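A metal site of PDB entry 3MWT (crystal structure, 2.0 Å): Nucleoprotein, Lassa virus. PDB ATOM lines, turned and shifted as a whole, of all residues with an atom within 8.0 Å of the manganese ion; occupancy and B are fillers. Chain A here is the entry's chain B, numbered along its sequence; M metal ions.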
ATOM      1  N   MET A 396      25.800 -18.625  12.691  1.00  0.00           N
ATOM      2  CA  MET A 396      25.441 -17.830  13.818  1.00  0.00           C
ATOM      3  C   MET A 396      25.253 -16.370  13.349  1.00  0.00           C
ATOM      4  O   MET A 396      25.929 -15.916  12.441  1.00  0.00           O
ATOM      5  CB  MET A 396      26.553 -17.922  14.909  1.00  0.00           C
ATOM      6  CG  MET A 396      26.272 -17.106  16.097  1.00  0.00           C
ATOM      7  SD  MET A 396      27.557 -17.239  17.348  1.00  0.00           S
ATOM      8  CE  MET A 396      26.965 -15.965  18.431  1.00  0.00           C
ATOM      9  N   ASP A 397      24.328 -15.692  14.004  1.00  0.00           N
ATOM     10  CA  ASP A 397      23.961 -14.313  13.679  1.00  0.00           C
ATOM     11  C   ASP A 397      23.465 -13.630  14.957  1.00  0.00           C
ATOM     12  O   ASP A 397      22.989 -14.278  15.916  1.00  0.00           O
ATOM     13  CB  ASP A 397      22.912 -14.291  12.560  1.00  0.00           C
ATOM     14  CG  ASP A 397      22.947 -12.978  11.734  1.00  0.00           C
ATOM     15  OD1 ASP A 397      22.056 -12.206  11.943  1.00  0.00           O
ATOM     16  OD2 ASP A 397      23.835 -12.738  10.897  1.00  0.00           O
ATOM     17  N   ILE A 398      23.592 -12.310  15.015  1.00  0.00           N
ATOM     18  CA  ILE A 398      23.077 -11.589  16.166  1.00  0.00           C
ATOM     19  C   ILE A 398      22.389 -10.312  15.772  1.00  0.00           C
ATOM     20  O   ILE A 398      22.698  -9.726  14.716  1.00  0.00           O
ATOM     21  CB  ILE A 398      24.183 -11.361  17.235  1.00  0.00           C
ATOM     22  CG1 ILE A 398      25.156 -10.273  16.760  1.00  0.00           C
ATOM     23  CG2 ILE A 398      24.927 -12.666  17.562  1.00  0.00           C
ATOM     24  CD1 ILE A 398      26.294  -9.922  17.800  1.00  0.00           C
ATOM     25  N   GLU A 399      21.424  -9.882  16.572  1.00  0.00           N
ATOM     26  CA  GLU A 399      20.984  -8.469  16.491  1.00  0.00           C
ATOM     27  C   GLU A 399      21.433  -7.722  17.725  1.00  0.00           C
ATOM     28  O   GLU A 399      21.565  -8.304  18.820  1.00  0.00           O
ATOM     29  CB  GLU A 399      19.468  -8.366  16.288  1.00  0.00           C
ATOM     30  CG  GLU A 399      18.942  -9.242  15.126  1.00  0.00           C
ATOM     31  CD  GLU A 399      19.606  -8.982  13.742  1.00  0.00           C
ATOM     32  OE1 GLU A 399      19.748  -7.817  13.352  1.00  0.00           O
ATOM     33  OE2 GLU A 399      19.888  -9.938  12.979  1.00  0.00           O
ATOM     34  N   GLY A 400      21.690  -6.413  17.576  1.00  0.00           N
ATOM     35  CA  GLY A 400      22.469  -5.712  18.639  1.00  0.00           C
ATOM     36  C   GLY A 400      23.914  -5.651  18.254  1.00  0.00           C
ATOM     37  O   GLY A 400      24.368  -6.419  17.392  1.00  0.00           O
ATOM     38  N   GLU A 407      19.616 -10.360  20.580  1.00  0.00           N
ATOM     39  CA  GLU A 407      19.095 -11.587  19.960  1.00  0.00           C
ATOM     40  C   GLU A 407      20.208 -12.382  19.404  1.00  0.00           C
ATOM     41  O   GLU A 407      21.019 -11.903  18.650  1.00  0.00           O
ATOM     42  CB  GLU A 407      18.046 -11.328  18.827  1.00  0.00           C
ATOM     43  CG  GLU A 407      17.360 -12.642  18.351  1.00  0.00           C
ATOM     44  CD  GLU A 407      16.308 -12.333  17.271  1.00  0.00           C
ATOM     45  OE1 GLU A 407      16.563 -11.458  16.413  1.00  0.00           O
ATOM     46  OE2 GLU A 407      15.271 -12.988  17.368  1.00  0.00           O
ATOM     47  N   SER A 438      17.133  -1.613  12.394  1.00  0.00           N
ATOM     48  CA  SER A 438      17.522  -2.990  12.236  1.00  0.00           C
ATOM     49  C   SER A 438      16.391  -3.905  12.592  1.00  0.00           C
ATOM     50  O   SER A 438      15.756  -4.464  11.695  1.00  0.00           O
ATOM     51  CB  SER A 438      18.749  -3.344  13.126  1.00  0.00           C
ATOM     52  OG  SER A 438      19.209  -4.631  12.734  1.00  0.00           O
ATOM     53  N   HIS A 439      16.106  -4.035  13.897  1.00  0.00           N
ATOM     54  CA  HIS A 439      15.462  -5.267  14.421  1.00  0.00           C
ATOM     55  C   HIS A 439      14.013  -5.082  14.905  1.00  0.00           C
ATOM     56  O   HIS A 439      13.265  -6.032  14.990  1.00  0.00           O
ATOM     57  CB  HIS A 439      16.361  -5.936  15.487  1.00  0.00           C
ATOM     58  CG  HIS A 439      16.658  -5.073  16.662  1.00  0.00           C
ATOM     59  ND1 HIS A 439      15.682  -4.464  17.426  1.00  0.00           N
ATOM     60  CD2 HIS A 439      17.854  -4.713  17.210  1.00  0.00           C
ATOM     61  CE1 HIS A 439      16.259  -3.787  18.398  1.00  0.00           C
ATOM     62  NE2 HIS A 439      17.574  -3.941  18.308  1.00  0.00           N
ATOM     63  N   GLN A 470      27.817 -14.115   8.314  1.00  0.00           N
ATOM     64  CA  GLN A 470      27.906 -12.955   7.439  1.00  0.00           C
ATOM     65  C   GLN A 470      28.702 -11.857   8.180  1.00  0.00           C
ATOM     66  O   GLN A 470      29.889 -11.576   7.840  1.00  0.00           O
ATOM     67  CB  GLN A 470      26.475 -12.558   7.014  1.00  0.00           C
ATOM     68  CG  GLN A 470      26.313 -11.255   6.221  1.00  0.00           C
ATOM     69  CD  GLN A 470      26.576 -11.403   4.738  1.00  0.00           C
ATOM     70  OE1 GLN A 470      27.408 -12.203   4.305  1.00  0.00           O
ATOM     71  NE2 GLN A 470      25.863 -10.618   3.955  1.00  0.00           N
ATOM     72  N   GLY A 471      28.078 -11.265   9.200  1.00  0.00           N
ATOM     73  CA  GLY A 471      28.825 -10.502  10.250  1.00  0.00           C
ATOM     74  C   GLY A 471      29.996 -11.250  10.877  1.00  0.00           C
ATOM     75  O   GLY A 471      29.834 -11.704  11.997  1.00  0.00           O
ATOM     76  N   ASP A 474      31.723  -9.049  14.107  1.00  0.00           N
ATOM     77  CA  ASP A 474      30.916  -8.803  15.260  1.00  0.00           C
ATOM     78  C   ASP A 474      30.763 -10.139  16.027  1.00  0.00           C
ATOM     79  O   ASP A 474      30.765 -10.104  17.245  1.00  0.00           O
ATOM     80  CB  ASP A 474      29.560  -8.214  14.890  1.00  0.00           C
ATOM     81  CG  ASP A 474      28.703  -9.206  14.086  1.00  0.00           C
ATOM     82  OD1 ASP A 474      29.231  -9.860  13.199  1.00  0.00           O
ATOM     83  OD2 ASP A 474      27.515  -9.341  14.352  1.00  0.00           O
ATOM     84  N   ARG A 500      19.885 -11.444   0.888  1.00  0.00           N
ATOM     85  CA  ARG A 500      18.448 -11.347   1.159  1.00  0.00           C
ATOM     86  C   ARG A 500      17.539 -11.854   0.047  1.00  0.00           C
ATOM     87  O   ARG A 500      16.324 -11.624   0.049  1.00  0.00           O
ATOM     88  CB  ARG A 500      18.108  -9.916   1.628  1.00  0.00           C
ATOM     89  CG  ARG A 500      18.897  -9.623   2.921  1.00  0.00           C
ATOM     90  CD  ARG A 500      18.210  -8.594   3.763  1.00  0.00           C
ATOM     91  NE  ARG A 500      18.960  -8.360   4.975  1.00  0.00           N
ATOM     92  CZ  ARG A 500      18.762  -9.025   6.123  1.00  0.00           C
ATOM     93  NH1 ARG A 500      17.792  -9.927   6.235  1.00  0.00           N
ATOM     94  NH2 ARG A 500      19.502  -8.727   7.160  1.00  0.00           N
ATOM     95  N   PRO A 535      11.954  -6.185   9.221  1.00  0.00           N
ATOM     96  CA  PRO A 535      12.935  -6.315  10.321  1.00  0.00           C
ATOM     97  C   PRO A 535      13.896  -7.505  10.213  1.00  0.00           C
ATOM     98  O   PRO A 535      13.573  -8.533   9.642  1.00  0.00           O
ATOM     99  CB  PRO A 535      12.075  -6.449  11.564  1.00  0.00           C
ATOM    100  CG  PRO A 535      10.701  -5.949  11.163  1.00  0.00           C
ATOM    101  CD  PRO A 535      10.565  -6.277   9.710  1.00  0.00           C
ATOM    102  N   HIS A 536      15.094  -7.315  10.768  1.00  0.00           N
ATOM    103  CA  HIS A 536      16.107  -8.348  10.793  1.00  0.00           C
ATOM    104  C   HIS A 536      15.934  -9.139  12.034  1.00  0.00           C
ATOM    105  O   HIS A 536      15.860  -8.584  13.167  1.00  0.00           O
ATOM    106  CB  HIS A 536      17.510  -7.711  10.754  1.00  0.00           C
ATOM    107  CG  HIS A 536      17.756  -6.933   9.507  1.00  0.00           C
ATOM    108  ND1 HIS A 536      18.952  -6.306   9.226  1.00  0.00           N
ATOM    109  CD2 HIS A 536      16.970  -6.742   8.427  1.00  0.00           C
ATOM    110  CE1 HIS A 536      18.871  -5.714   8.045  1.00  0.00           C
ATOM    111  NE2 HIS A 536      17.676  -5.969   7.536  1.00  0.00           N
ATOM    112  N   CYS A 537      15.951 -10.429  11.831  1.00  0.00           N
ATOM    113  CA  CYS A 537      15.821 -11.411  12.932  1.00  0.00           C
ATOM    114  C   CYS A 537      17.009 -12.331  12.752  1.00  0.00           C
ATOM    115  O   CYS A 537      17.287 -12.808  11.630  1.00  0.00           O
ATOM    116  CB  CYS A 537      14.512 -12.191  12.792  1.00  0.00           C
ATOM    117  SG  CYS A 537      14.575 -13.899  13.695  1.00  0.00           S
ATOM    118  N   ALA A 538      17.740 -12.519  13.847  1.00  0.00           N
ATOM    119  CA  ALA A 538      18.981 -13.288  13.837  1.00  0.00           C
ATOM    120  C   ALA A 538      18.680 -14.726  13.326  1.00  0.00           C
ATOM    121  O   ALA A 538      19.456 -15.280  12.536  1.00  0.00           O
ATOM    122  CB  ALA A 538      19.604 -13.300  15.313  1.00  0.00           C
ATOM    123  N   LEU A 539      17.559 -15.295  13.728  1.00  0.00           N
ATOM    124  CA  LEU A 539      17.227 -16.672  13.282  1.00  0.00           C
ATOM    125  C   LEU A 539      16.898 -16.742  11.778  1.00  0.00           C
ATOM    126  O   LEU A 539      17.555 -17.466  11.016  1.00  0.00           O
ATOM    127  CB  LEU A 539      16.104 -17.238  14.141  1.00  0.00           C
ATOM    128  CG  LEU A 539      15.544 -18.581  13.679  1.00  0.00           C
ATOM    129  CD1 LEU A 539      16.702 -19.582  13.775  1.00  0.00           C
ATOM    130  CD2 LEU A 539      14.355 -18.974  14.566  1.00  0.00           C
ATOM    131  N   MET A 540      15.890 -15.955  11.346  1.00  0.00           N
ATOM    132  CA  MET A 540      15.616 -15.793   9.904  1.00  0.00           C
ATOM    133  C   MET A 540      16.892 -15.467   9.107  1.00  0.00           C
ATOM    134  O   MET A 540      17.094 -16.026   8.039  1.00  0.00           O
ATOM    135  CB  MET A 540      14.506 -14.755   9.631  1.00  0.00           C
ATOM    136  CG  MET A 540      13.120 -15.040  10.275  1.00  0.00           C
ATOM    137  SD  MET A 540      12.616 -16.760  10.452  1.00  0.00           S
ATOM    138  CE  MET A 540      11.605 -16.685  11.923  1.00  0.00           C
ATOM    139  N   ASP A 541      17.758 -14.569   9.604  1.00  0.00           N
ATOM    140  CA  ASP A 541      18.987 -14.277   8.891  1.00  0.00           C
ATOM    141  C   ASP A 541      19.900 -15.503   8.653  1.00  0.00           C
ATOM    142  O   ASP A 541      20.393 -15.705   7.551  1.00  0.00           O
ATOM    143  CB  ASP A 541      19.775 -13.150   9.613  1.00  0.00           C
ATOM    144  CG  ASP A 541      19.168 -11.784   9.336  1.00  0.00           C
ATOM    145  OD1 ASP A 541      18.229 -11.669   8.518  1.00  0.00           O
ATOM    146  OD2 ASP A 541      19.644 -10.845   9.925  1.00  0.00           O
ATOM    147  N   CYS A 542      20.104 -16.321   9.671  1.00  0.00           N
ATOM    148  CA  CYS A 542      20.837 -17.581   9.494  1.00  0.00           C
ATOM    149  C   CYS A 542      20.220 -18.443   8.380  1.00  0.00           C
ATOM    150  O   CYS A 542      20.921 -18.956   7.491  1.00  0.00           O
ATOM    151  CB  CYS A 542      20.828 -18.351  10.813  1.00  0.00           C
ATOM    152  SG  CYS A 542      21.948 -17.719  12.140  1.00  0.00           S
ATOM    153  N   MET A 544      18.069 -17.674   5.942  1.00  0.00           N
ATOM    154  CA  MET A 544      18.130 -17.060   4.601  1.00  0.00           C
ATOM    155  C   MET A 544      19.539 -17.048   4.057  1.00  0.00           C
ATOM    156  O   MET A 544      19.700 -17.292   2.883  1.00  0.00           O
ATOM    157  CB  MET A 544      17.444 -15.664   4.531  1.00  0.00           C
ATOM    158  CG  MET A 544      18.219 -14.448   5.066  1.00  0.00           C
ATOM    159  SD  MET A 544      17.236 -12.927   4.822  1.00  0.00           S
ATOM    160  CE  MET A 544      15.903 -13.133   5.987  1.00  0.00           C
ATOM    161  N   PHE A 545      20.557 -16.825   4.907  1.00  0.00           N
ATOM    162  CA  PHE A 545      21.948 -16.936   4.422  1.00  0.00           C
ATOM    163  C   PHE A 545      22.323 -18.333   3.918  1.00  0.00           C
ATOM    164  O   PHE A 545      22.913 -18.481   2.811  1.00  0.00           O
ATOM    165  CB  PHE A 545      22.992 -16.352   5.407  1.00  0.00           C
ATOM    166  CG  PHE A 545      22.658 -14.939   5.903  1.00  0.00           C
ATOM    167  CD1 PHE A 545      21.946 -14.042   5.109  1.00  0.00           C
ATOM    168  CD2 PHE A 545      23.086 -14.514   7.179  1.00  0.00           C
ATOM    169  CE1 PHE A 545      21.629 -12.757   5.582  1.00  0.00           C
ATOM    170  CE2 PHE A 545      22.799 -13.219   7.635  1.00  0.00           C
ATOM    171  CZ  PHE A 545      22.050 -12.349   6.840  1.00  0.00           C
HETATM  172 MN    MN M   1      21.221 -10.303  11.114  1.00  0.00          MN
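Residues that only touch the manganese ion: Ile 398.
Of the 22 residues printed, 4 come within 4 Å of the manganese ion.
The nearest printed residue that does not touch the manganese ion is His 536 (4.5 Å).
The manganese ion is bound by the side-chain carboxylate (OD2) of Asp 541 (2.0 Å), the side-chain carboxylate (OD1) of Asp 397 (2.2 Å) and the side-chain carboxylate (OE2) of Glu 399 (2.3 Å).
The guanidinium group (NH1) of Arg 500 lies within salt-bridge range of the side-chain carboxylate (OD1) of Asp 541, at 2.9 Å.
N of Asp 397 sits close to SG of Cys 542.
The side-chain carboxylate (OE2) of Glu 399 sits close to the backbone NH (N) of Ala 538 (3.5 Å).
The side-chain carboxylate of Glu 399 sits at hydrogen-bond distance from the side-chain hydroxyl of Ser 438 (3.3 Å).
The backbone NH of Glu 399 sits at hydrogen-bond distance from the backbone carbonyl oxygen of Glu 407 (2.9 Å).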
